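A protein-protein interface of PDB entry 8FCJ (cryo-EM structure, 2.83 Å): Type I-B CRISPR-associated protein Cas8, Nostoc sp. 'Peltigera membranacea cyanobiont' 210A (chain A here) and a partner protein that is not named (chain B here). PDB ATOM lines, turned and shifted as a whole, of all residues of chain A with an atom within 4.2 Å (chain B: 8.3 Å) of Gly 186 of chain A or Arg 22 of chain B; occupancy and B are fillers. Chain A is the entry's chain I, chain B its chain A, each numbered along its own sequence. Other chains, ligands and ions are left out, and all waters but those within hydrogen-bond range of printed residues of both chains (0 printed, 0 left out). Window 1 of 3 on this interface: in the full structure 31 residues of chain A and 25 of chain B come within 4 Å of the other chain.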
ATOM      1  N   TYR A 184      18.382  24.177  11.816  1.00  0.00           N
ATOM      2  CA  TYR A 184      18.407  23.601  10.480  1.00  0.00           C
ATOM      3  C   TYR A 184      17.088  22.881  10.244  1.00  0.00           C
ATOM      4  O   TYR A 184      16.786  21.898  10.926  1.00  0.00           O
ATOM      5  CB  TYR A 184      19.581  22.638  10.330  1.00  0.00           C
ATOM      6  CG  TYR A 184      20.074  22.472   8.913  1.00  0.00           C
ATOM      7  CD1 TYR A 184      19.278  21.877   7.948  1.00  0.00           C
ATOM      8  CD2 TYR A 184      21.336  22.906   8.544  1.00  0.00           C
ATOM      9  CE1 TYR A 184      19.725  21.723   6.655  1.00  0.00           C
ATOM     10  CE2 TYR A 184      21.792  22.757   7.254  1.00  0.00           C
ATOM     11  CZ  TYR A 184      20.982  22.165   6.312  1.00  0.00           C
ATOM     12  OH  TYR A 184      21.432  22.013   5.022  1.00  0.00           O
ATOM     13  N   LEU A 185      16.304  23.373   9.289  1.00  0.00           N
ATOM     14  CA  LEU A 185      15.027  22.744   8.985  1.00  0.00           C
ATOM     15  C   LEU A 185      15.247  21.314   8.516  1.00  0.00           C
ATOM     16  O   LEU A 185      16.048  21.058   7.613  1.00  0.00           O
ATOM     17  CB  LEU A 185      14.283  23.545   7.919  1.00  0.00           C
ATOM     18  CG  LEU A 185      13.848  24.954   8.316  1.00  0.00           C
ATOM     19  CD1 LEU A 185      12.944  25.548   7.255  1.00  0.00           C
ATOM     20  CD2 LEU A 185      13.153  24.931   9.662  1.00  0.00           C
ATOM     21  N   GLY A 186      14.534  20.379   9.136  1.00  0.00           N
ATOM     22  CA  GLY A 186      14.703  18.977   8.836  1.00  0.00           C
ATOM     23  C   GLY A 186      15.827  18.295   9.581  1.00  0.00           C
ATOM     24  O   GLY A 186      15.976  17.073   9.457  1.00  0.00           O
ATOM     25  N   GLY A 187      16.616  19.035  10.357  1.00  0.00           N
ATOM     26  CA  GLY A 187      17.687  18.442  11.133  1.00  0.00           C
ATOM     27  C   GLY A 187      17.169  17.740  12.368  1.00  0.00           C
ATOM     28  O   GLY A 187      17.597  18.027  13.489  1.00  0.00           O
ATOM     29  N   ILE A 188      16.251  16.817  12.168  1.00  0.00           N
ATOM     30  CA  ILE A 188      15.559  16.134  13.250  1.00  0.00           C
ATOM     31  C   ILE A 188      16.499  15.113  13.871  1.00  0.00           C
ATOM     32  O   ILE A 188      17.494  14.700  13.265  1.00  0.00           O
ATOM     33  CB  ILE A 188      14.265  15.472  12.727  1.00  0.00           C
ATOM     34  CG1 ILE A 188      13.134  15.641  13.734  1.00  0.00           C
ATOM     35  CG2 ILE A 188      14.484  14.001  12.418  1.00  0.00           C
ATOM     36  CD1 ILE A 188      12.745  17.077  13.932  1.00  0.00           C
ATOM     37  N   ARG A 190      16.360  11.466  14.636  1.00  0.00           N
ATOM     38  CA  ARG A 190      15.502  10.342  14.277  1.00  0.00           C
ATOM     39  C   ARG A 190      15.237   9.442  15.475  1.00  0.00           C
ATOM     40  O   ARG A 190      14.097   9.029  15.717  1.00  0.00           O
ATOM     41  CB  ARG A 190      16.132   9.542  13.139  1.00  0.00           C
ATOM     42  CG  ARG A 190      16.779  10.382  12.061  1.00  0.00           C
ATOM     43  CD  ARG A 190      16.134  10.114  10.716  1.00  0.00           C
ATOM     44  NE  ARG A 190      15.842   8.699  10.523  1.00  0.00           N
ATOM     45  CZ  ARG A 190      16.528   7.894   9.722  1.00  0.00           C
ATOM     46  NH1 ARG A 190      17.561   8.332   9.024  1.00  0.00           N
ATOM     47  NH2 ARG A 190      16.166   6.619   9.621  1.00  0.00           N
ATOM     48  N   THR A 198      23.483  11.326  18.425  1.00  0.00           N
ATOM     49  CA  THR A 198      22.990  11.469  17.054  1.00  0.00           C
ATOM     50  C   THR A 198      22.284  12.815  16.896  1.00  0.00           C
ATOM     51  O   THR A 198      21.063  12.914  16.763  1.00  0.00           O
ATOM     52  CB  THR A 198      22.070  10.313  16.693  1.00  0.00           C
ATOM     53  OG1 THR A 198      20.905  10.350  17.526  1.00  0.00           O
ATOM     54  CG2 THR A 198      22.783   8.988  16.890  1.00  0.00           C
ATOM     55  N   LYS A 199      23.091  13.870  16.906  1.00  0.00           N
ATOM     56  CA  LYS A 199      22.616  15.231  16.712  1.00  0.00           C
ATOM     57  C   LYS A 199      23.498  15.909  15.678  1.00  0.00           C
ATOM     58  O   LYS A 199      24.720  15.735  15.688  1.00  0.00           O
ATOM     59  CB  LYS A 199      22.640  16.020  18.022  1.00  0.00           C
ATOM     60  CG  LYS A 199      21.349  16.737  18.349  1.00  0.00           C
ATOM     61  CD  LYS A 199      21.222  16.945  19.846  1.00  0.00           C
ATOM     62  CE  LYS A 199      20.086  17.888  20.186  1.00  0.00           C
ATOM     63  NZ  LYS A 199      19.933  18.042  21.657  1.00  0.00           N
ATOM     64  N   LEU A 200      22.880  16.673  14.781  1.00  0.00           N
ATOM     65  CA  LEU A 200      23.646  17.389  13.770  1.00  0.00           C
ATOM     66  C   LEU A 200      24.549  18.421  14.430  1.00  0.00           C
ATOM     67  O   LEU A 200      24.123  19.154  15.326  1.00  0.00           O
ATOM     68  CB  LEU A 200      22.705  18.062  12.772  1.00  0.00           C
ATOM     69  CG  LEU A 200      22.013  17.135  11.774  1.00  0.00           C
ATOM     70  CD1 LEU A 200      21.305  17.940  10.703  1.00  0.00           C
ATOM     71  CD2 LEU A 200      23.007  16.172  11.153  1.00  0.00           C
ATOM     72  N   TYR A 298       5.244  22.231   4.965  1.00  0.00           N
ATOM     73  CA  TYR A 298       5.031  21.881   6.363  1.00  0.00           C
ATOM     74  C   TYR A 298       3.537  21.711   6.592  1.00  0.00           C
ATOM     75  O   TYR A 298       2.759  22.635   6.339  1.00  0.00           O
ATOM     76  CB  TYR A 298       5.611  22.948   7.288  1.00  0.00           C
ATOM     77  CG  TYR A 298       7.079  22.751   7.564  1.00  0.00           C
ATOM     78  CD1 TYR A 298       8.033  23.107   6.626  1.00  0.00           C
ATOM     79  CD2 TYR A 298       7.509  22.194   8.758  1.00  0.00           C
ATOM     80  CE1 TYR A 298       9.374  22.922   6.870  1.00  0.00           C
ATOM     81  CE2 TYR A 298       8.848  22.006   9.010  1.00  0.00           C
ATOM     82  CZ  TYR A 298       9.776  22.371   8.064  1.00  0.00           C
ATOM     83  OH  TYR A 298      11.112  22.184   8.316  1.00  0.00           O
ATOM     84  N   ARG B  17      20.239   9.694   0.347  1.00  0.00           N
ATOM     85  CA  ARG B  17      19.731  10.660   1.322  1.00  0.00           C
ATOM     86  C   ARG B  17      20.747  11.745   1.655  1.00  0.00           C
ATOM     87  O   ARG B  17      21.953  11.498   1.659  1.00  0.00           O
ATOM     88  CB  ARG B  17      19.297   9.946   2.606  1.00  0.00           C
ATOM     89  CG  ARG B  17      18.632  10.854   3.628  1.00  0.00           C
ATOM     90  CD  ARG B  17      17.642  10.086   4.487  1.00  0.00           C
ATOM     91  NE  ARG B  17      16.597  10.952   5.024  1.00  0.00           N
ATOM     92  CZ  ARG B  17      15.846  10.655   6.080  1.00  0.00           C
ATOM     93  NH1 ARG B  17      16.021   9.509   6.720  1.00  0.00           N
ATOM     94  NH2 ARG B  17      14.921  11.508   6.498  1.00  0.00           N
ATOM     95  N   GLU B  18      20.263  12.950   1.939  1.00  0.00           N
ATOM     96  CA  GLU B  18      21.165  14.038   2.304  1.00  0.00           C
ATOM     97  C   GLU B  18      21.612  13.923   3.745  1.00  0.00           C
ATOM     98  O   GLU B  18      20.901  13.365   4.583  1.00  0.00           O
ATOM     99  CB  GLU B  18      20.514  15.404   2.068  1.00  0.00           C
ATOM    100  CG  GLU B  18      19.432  15.415   1.004  1.00  0.00           C
ATOM    101  CD  GLU B  18      19.959  15.120  -0.385  1.00  0.00           C
ATOM    102  OE1 GLU B  18      19.791  15.974  -1.279  1.00  0.00           O
ATOM    103  OE2 GLU B  18      20.535  14.033  -0.589  1.00  0.00           O
ATOM    104  N   SER B  19      22.787  14.459   4.040  1.00  0.00           N
ATOM    105  CA  SER B  19      23.333  14.375   5.390  1.00  0.00           C
ATOM    106  C   SER B  19      22.417  15.044   6.406  1.00  0.00           C
ATOM    107  O   SER B  19      22.187  14.505   7.495  1.00  0.00           O
ATOM    108  CB  SER B  19      24.721  15.006   5.427  1.00  0.00           C
ATOM    109  OG  SER B  19      25.568  14.409   4.462  1.00  0.00           O
ATOM    110  N   HIS B  20      21.885  16.213   6.070  1.00  0.00           N
ATOM    111  CA  HIS B  20      21.025  16.959   6.977  1.00  0.00           C
ATOM    112  C   HIS B  20      19.549  16.655   6.779  1.00  0.00           C
ATOM    113  O   HIS B  20      18.712  17.261   7.456  1.00  0.00           O
ATOM    114  CB  HIS B  20      21.269  18.460   6.809  1.00  0.00           C
ATOM    115  CG  HIS B  20      22.715  18.842   6.848  1.00  0.00           C
ATOM    116  ND1 HIS B  20      23.374  19.142   8.020  1.00  0.00           N
ATOM    117  CD2 HIS B  20      23.630  18.969   5.859  1.00  0.00           C
ATOM    118  CE1 HIS B  20      24.632  19.439   7.750  1.00  0.00           C
ATOM    119  NE2 HIS B  20      24.813  19.343   6.446  1.00  0.00           N
ATOM    120  N   ALA B  21      19.207  15.741   5.875  1.00  0.00           N
ATOM    121  CA  ALA B  21      17.814  15.393   5.608  1.00  0.00           C
ATOM    122  C   ALA B  21      17.429  14.234   6.515  1.00  0.00           C
ATOM    123  O   ALA B  21      17.513  13.066   6.139  1.00  0.00           O
ATOM    124  CB  ALA B  21      17.615  15.048   4.140  1.00  0.00           C
ATOM    125  N   ARG B  22      17.000  14.562   7.732  1.00  0.00           N
ATOM    126  CA  ARG B  22      16.559  13.560   8.690  1.00  0.00           C
ATOM    127  C   ARG B  22      15.056  13.539   8.902  1.00  0.00           C
ATOM    128  O   ARG B  22      14.502  12.471   9.165  1.00  0.00           O
ATOM    129  CB  ARG B  22      17.253  13.774  10.040  1.00  0.00           C
ATOM    130  CG  ARG B  22      18.662  13.215  10.087  1.00  0.00           C
ATOM    131  CD  ARG B  22      19.615  14.167  10.774  1.00  0.00           C
ATOM    132  NE  ARG B  22      19.790  13.837  12.183  1.00  0.00           N
ATOM    133  CZ  ARG B  22      20.877  13.276  12.689  1.00  0.00           C
ATOM    134  NH1 ARG B  22      21.911  12.960  11.926  1.00  0.00           N
ATOM    135  NH2 ARG B  22      20.932  13.024  13.993  1.00  0.00           N
ATOM    136  N   GLU B  23      14.382  14.684   8.793  1.00  0.00           N
ATOM    137  CA  GLU B  23      12.929  14.687   8.903  1.00  0.00           C
ATOM    138  C   GLU B  23      12.272  14.132   7.649  1.00  0.00           C
ATOM    139  O   GLU B  23      11.205  13.517   7.733  1.00  0.00           O
ATOM    140  CB  GLU B  23      12.422  16.099   9.186  1.00  0.00           C
ATOM    141  CG  GLU B  23      10.973  16.150   9.633  1.00  0.00           C
ATOM    142  CD  GLU B  23      10.597  17.485  10.238  1.00  0.00           C
ATOM    143  OE1 GLU B  23      11.373  18.450  10.079  1.00  0.00           O
ATOM    144  OE2 GLU B  23       9.529  17.571  10.876  1.00  0.00           O
ATOM    145  N   MET B  24      12.881  14.345   6.486  1.00  0.00           N
ATOM    146  CA  MET B  24      12.377  13.832   5.222  1.00  0.00           C
ATOM    147  C   MET B  24      13.534  13.250   4.425  1.00  0.00           C
ATOM    148  O   MET B  24      14.649  13.776   4.462  1.00  0.00           O
ATOM    149  CB  MET B  24      11.678  14.927   4.415  1.00  0.00           C
ATOM    150  CG  MET B  24      10.902  14.418   3.219  1.00  0.00           C
ATOM    151  SD  MET B  24      11.047  15.504   1.793  1.00  0.00           S
ATOM    152  CE  MET B  24      10.534  14.402   0.483  1.00  0.00           C
ATOM    153  N   GLY B  25      13.265  12.167   3.702  1.00  0.00           N
ATOM    154  CA  GLY B  25      14.307  11.481   2.965  1.00  0.00           C
ATOM    155  C   GLY B  25      14.653  12.105   1.630  1.00  0.00           C
ATOM    156  O   GLY B  25      14.414  11.504   0.580  1.00  0.00           O
ATOM    157  N   LYS B  26      15.217  13.309   1.655  1.00  0.00           N
ATOM    158  CA  LYS B  26      15.653  13.955   0.426  1.00  0.00           C
ATOM    159  C   LYS B  26      16.907  13.274  -0.109  1.00  0.00           C
ATOM    160  O   LYS B  26      17.789  12.878   0.656  1.00  0.00           O
ATOM    161  CB  LYS B  26      15.920  15.437   0.677  1.00  0.00           C
ATOM    162  CG  LYS B  26      16.248  16.231  -0.569  1.00  0.00           C
ATOM    163  CD  LYS B  26      16.528  17.682  -0.235  1.00  0.00           C
ATOM    164  CE  LYS B  26      16.769  18.494  -1.494  1.00  0.00           C
ATOM    165  NZ  LYS B  26      16.285  17.782  -2.707  1.00  0.00           N
ATOM    166  N   MET B  74       8.882   3.822   8.271  1.00  0.00           N
ATOM    167  CA  MET B  74      10.195   3.550   8.835  1.00  0.00           C
ATOM    168  C   MET B  74      10.153   3.569  10.356  1.00  0.00           C
ATOM    169  O   MET B  74       9.414   4.345  10.968  1.00  0.00           O
ATOM    170  CB  MET B  74      11.233   4.549   8.322  1.00  0.00           C
ATOM    171  CG  MET B  74      11.212   4.783   6.826  1.00  0.00           C
ATOM    172  SD  MET B  74      11.792   6.427   6.395  1.00  0.00           S
ATOM    173  CE  MET B  74      10.316   7.360   6.728  1.00  0.00           C
ATOM    174  N   ARG B  76      12.136   3.665  14.258  1.00  0.00           N
ATOM    175  CA  ARG B  76      13.167   4.445  14.923  1.00  0.00           C
ATOM    176  C   ARG B  76      13.225   4.031  16.384  1.00  0.00           C
ATOM    177  O   ARG B  76      12.302   3.404  16.908  1.00  0.00           O
ATOM    178  CB  ARG B  76      12.910   5.949  14.794  1.00  0.00           C
ATOM    179  CG  ARG B  76      11.803   6.468  15.688  1.00  0.00           C
ATOM    180  CD  ARG B  76      10.528   6.695  14.905  1.00  0.00           C
ATOM    181  NE  ARG B  76       9.490   7.315  15.718  1.00  0.00           N
ATOM    182  CZ  ARG B  76       9.134   8.588  15.631  1.00  0.00           C
ATOM    183  NH1 ARG B  76       9.726   9.414  14.784  1.00  0.00           N
ATOM    184  NH2 ARG B  76       8.163   9.045  16.414  1.00  0.00           N
ATOM    185  N   ILE B  89       7.024   5.689  12.412  1.00  0.00           N
ATOM    186  CA  ILE B  89       6.644   7.006  11.909  1.00  0.00           C
ATOM    187  C   ILE B  89       6.522   6.944  10.391  1.00  0.00           C
ATOM    188  O   ILE B  89       7.362   6.326   9.723  1.00  0.00           O
ATOM    189  CB  ILE B  89       7.650   8.084  12.350  1.00  0.00           C
ATOM    190  CG1 ILE B  89       7.184   9.469  11.905  1.00  0.00           C
ATOM    191  CG2 ILE B  89       9.038   7.791  11.807  1.00  0.00           C
ATOM    192  CD1 ILE B  89       6.139  10.078  12.804  1.00  0.00           C
ATOM    193  N   CYS B  91       6.989   8.697   6.878  1.00  0.00           N
ATOM    194  CA  CYS B  91       7.601   9.848   6.233  1.00  0.00           C
ATOM    195  C   CYS B  91       8.043   9.455   4.834  1.00  0.00           C
ATOM    196  O   CYS B  91       8.202   8.271   4.525  1.00  0.00           O
ATOM    197  CB  CYS B  91       8.781  10.393   7.041  1.00  0.00           C
ATOM    198  SG  CYS B  91       9.988  11.272   6.039  1.00  0.00           S
ATOM    199  N   TYR B  92       8.224  10.461   3.987  1.00  0.00           N
ATOM    200  CA  TYR B  92       8.537  10.232   2.586  1.00  0.00           C
ATOM    201  C   TYR B  92      10.023   9.972   2.384  1.00  0.00           C
ATOM    202  O   TYR B  92      10.875  10.493   3.108  1.00  0.00           O
ATOM    203  CB  TYR B  92       8.105  11.427   1.743  1.00  0.00           C
ATOM    204  CG  TYR B  92       6.629  11.444   1.439  1.00  0.00           C
ATOM    205  CD1 TYR B  92       6.062  10.488   0.612  1.00  0.00           C
ATOM    206  CD2 TYR B  92       5.800  12.407   1.991  1.00  0.00           C
ATOM    207  CE1 TYR B  92       4.714  10.498   0.333  1.00  0.00           C
ATOM    208  CE2 TYR B  92       4.450  12.424   1.719  1.00  0.00           C
ATOM    209  CZ  TYR B  92       3.912  11.468   0.890  1.00  0.00           C
ATOM    210  OH  TYR B  92       2.565  11.485   0.618  1.00  0.00           O
ATOM    211  N   ASP B 178      29.969  10.592   8.571  1.00  0.00           N
ATOM    212  CA  ASP B 178      29.887  10.217   9.976  1.00  0.00           C
ATOM    213  C   ASP B 178      28.450   9.769  10.207  1.00  0.00           C
ATOM    214  O   ASP B 178      27.525  10.586  10.167  1.00  0.00           O
ATOM    215  CB  ASP B 178      30.277  11.392  10.875  1.00  0.00           C
ATOM    216  CG  ASP B 178      29.950  11.168  12.354  1.00  0.00           C
ATOM    217  OD1 ASP B 178      29.349  10.142  12.730  1.00  0.00           O
ATOM    218  OD2 ASP B 178      30.303  12.052  13.161  1.00  0.00           O
ATOM    219  N   HIS B 179      28.262   8.474  10.449  1.00  0.00           N
ATOM    220  CA  HIS B 179      26.922   7.919  10.579  1.00  0.00           C
ATOM    221  C   HIS B 179      26.297   8.172  11.942  1.00  0.00           C
ATOM    222  O   HIS B 179      25.089   7.963  12.096  1.00  0.00           O
ATOM    223  CB  HIS B 179      26.956   6.418  10.296  1.00  0.00           C
ATOM    224  CG  HIS B 179      27.551   6.075   8.968  1.00  0.00           C
ATOM    225  ND1 HIS B 179      28.868   5.700   8.818  1.00  0.00           N
ATOM    226  CD2 HIS B 179      27.011   6.060   7.728  1.00  0.00           C
ATOM    227  CE1 HIS B 179      29.112   5.463   7.541  1.00  0.00           C
ATOM    228  NE2 HIS B 179      28.001   5.674   6.859  1.00  0.00           N
ATOM    229  N   VAL B 180      27.074   8.613  12.928  1.00  0.00           N
ATOM    230  CA  VAL B 180      26.513   8.897  14.245  1.00  0.00           C
ATOM    231  C   VAL B 180      25.891  10.286  14.274  1.00  0.00           C
ATOM    232  O   VAL B 180      24.681  10.442  14.473  1.00  0.00           O
ATOM    233  CB  VAL B 180      27.592   8.744  15.332  1.00  0.00           C
ATOM    234  CG1 VAL B 180      26.977   8.899  16.709  1.00  0.00           C
ATOM    235  CG2 VAL B 180      28.283   7.401  15.199  1.00  0.00           C
ATOM    236  N   GLY B 181      26.707  11.313  14.061  1.00  0.00           N
ATOM    237  CA  GLY B 181      26.212  12.672  13.990  1.00  0.00           C
ATOM    238  C   GLY B 181      26.582  13.330  12.678  1.00  0.00           C
ATOM    239  O   GLY B 181      26.249  12.820  11.606  1.00  0.00           O
ATOM    240  N   SER B 182      27.265  14.472  12.751  1.00  0.00           N
ATOM    241  CA  SER B 182      27.781  15.115  11.551  1.00  0.00           C
ATOM    242  C   SER B 182      29.171  15.701  11.763  1.00  0.00           C
ATOM    243  O   SER B 182      29.647  16.450  10.900  1.00  0.00           O
ATOM    244  CB  SER B 182      26.824  16.211  11.071  1.00  0.00           C
ATOM    245  OG  SER B 182      26.789  17.291  11.985  1.00  0.00           O
ATOM    246  N   THR B 185      31.729  14.209   9.166  1.00  0.00           N
ATOM    247  CA  THR B 185      31.339  14.253   7.764  1.00  0.00           C
ATOM    248  C   THR B 185      32.068  15.387   7.057  1.00  0.00           C
ATOM    249  O   THR B 185      32.120  16.513   7.558  1.00  0.00           O
ATOM    250  CB  THR B 185      29.829  14.434   7.639  1.00  0.00           C
ATOM    251  OG1 THR B 185      29.162  13.391   8.357  1.00  0.00           O
ATOM    252  CG2 THR B 185      29.407  14.380   6.185  1.00  0.00           C
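Of the 21 printed residues of chain B, 8 touch a printed residue of chain A. Hydrophobic or aromatic side chains of chain B within 4 Å of the printed part of chain A: His 20. Of the 10 printed residues of chain A, 8 touch a printed residue of chain B. Printed residues of chain A that touch a printed residue of chain B: Tyr 184, Gly 186, Gly 187, Ile 188, Arg 190, Thr 198, Lys 199 and Leu 200. Hydrophobic or aromatic side chains of chain A within 4 Å of the printed part of chain B: Tyr 184, Ile 188 and Leu 200. Among the printed residues, no Asp or Glu carboxylate lies within 4 Å of a Lys or Arg side-chain nitrogen of the other chain.
NH2 of Arg 22 of chain B sits at hydrogen-bond distance from O of Thr 198 of chain A, 2.8 Å away. The backbone carbonyl oxygen (O) of Gly 186 of chain A lies within hydrogen-bond range of the backbone NH (N) of Glu 23 of chain B (2.9 Å). NE of Arg 22 of chain B is in hydrogen-bond range of O of Ile 188 of chain A. The backbone carbonyl oxygen of Gly 186 of chain A lies close to the backbone carbonyl oxygen of His 20 of chain B, at 3.4 Å. NH1 of Arg 190 of chain A lies close to NH1 of Arg 17 of chain B, at 3.0 Å. The backbone carbonyl oxygen of Gly 186 of chain A is in hydrogen-bond range of the backbone NH of Arg 22 of chain B (3.2 Å).
The guanidinium group (NH2) of Arg 17 of chain B lies close to the backbone carbonyl oxygen (O) of Met 24 of chain B, at 3.1 Å. The side-chain carboxylate (OD1) of Asp 178 of chain B sits at hydrogen-bond distance from the backbone NH (N) of Val 180 of chain B (2.7 Å). NE of Arg 17 of chain B sits at hydrogen-bond distance from O of Ala 21 of chain B, 2.6 Å away. The guanidinium group of Arg 17 of chain B lies within hydrogen-bond range of the backbone carbonyl oxygen of Arg 22 of chain B. The side-chain sulfur (SG) of Cys 91 of chain B lies within hydrogen-bond range of the backbone carbonyl oxygen (O) of Glu 23 of chain B, 3.1 Å away. N of Gly 181 of chain B is in hydrogen-bond range of OD1 of Asp 178 of chain B (3.2 Å).
Among the printed residues, merely in contact across the chains: Tyr 184 of chain A with His 20 of chain B (3.6 Å), Gly 187 of chain A with His 20 of chain B (3.99 Å), Ile 188 of chain A with Glu 23 of chain B (3.7 Å), Arg 190 of chain A with Arg 22 of chain B (3.3 Å), Arg 190 of chain A with Arg 76 of chain B (3.4 Å), Thr 198 of chain A with Val 180 of chain B (3.3 Å), Lys 199 of chain A with Arg 22 of chain B (3.7 Å), Lys 199 of chain A with Gly 181 of chain B (3.8 Å), Leu 200 of chain A with His 20 of chain B (3.6 Å), Leu 200 of chain A with Arg 22 of chain B (3.5 Å) and Leu 200 of chain A with Ser 182 of chain B (3.5 Å).
Gly 186 of chain A touches just these residues of chain B: His 20, Arg 22 and Glu 23. Of the printed residues of chain B, Lys 199 of chain A touches Arg 22 (3.7 Å) and Gly 181 (3.8 Å). Of the printed residues of chain B, Leu 200 of chain A touches His 20, Arg 22 and Ser 182. Of chain A, only Gly 186 (3.2 Å), Ile 188 (2.7 Å), Arg 190 (3.3 Å), Thr 198 (2.8 Å), Lys 199 (3.7 Å) and Leu 200 (3.5 Å) come within 4 Å of Arg 22 of chain B. Of the printed residues of chain A, Arg 76 of chain B touches Arg 190 (3.4 Å). Thr 185 of chain B touches none of the printed residues of chain A. The nearest residue of chain B that does not touch Gly 186 of chain A is Ala 21 of chain B (4.3 Å). The nearest printed residue of chain A that does not touch Arg 22 of chain B is Gly 187 of chain A (4.6 Å). The nearest printed residue of chain B that does not touch Ile 188 of chain A is His 20 of chain B (5.3 Å).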
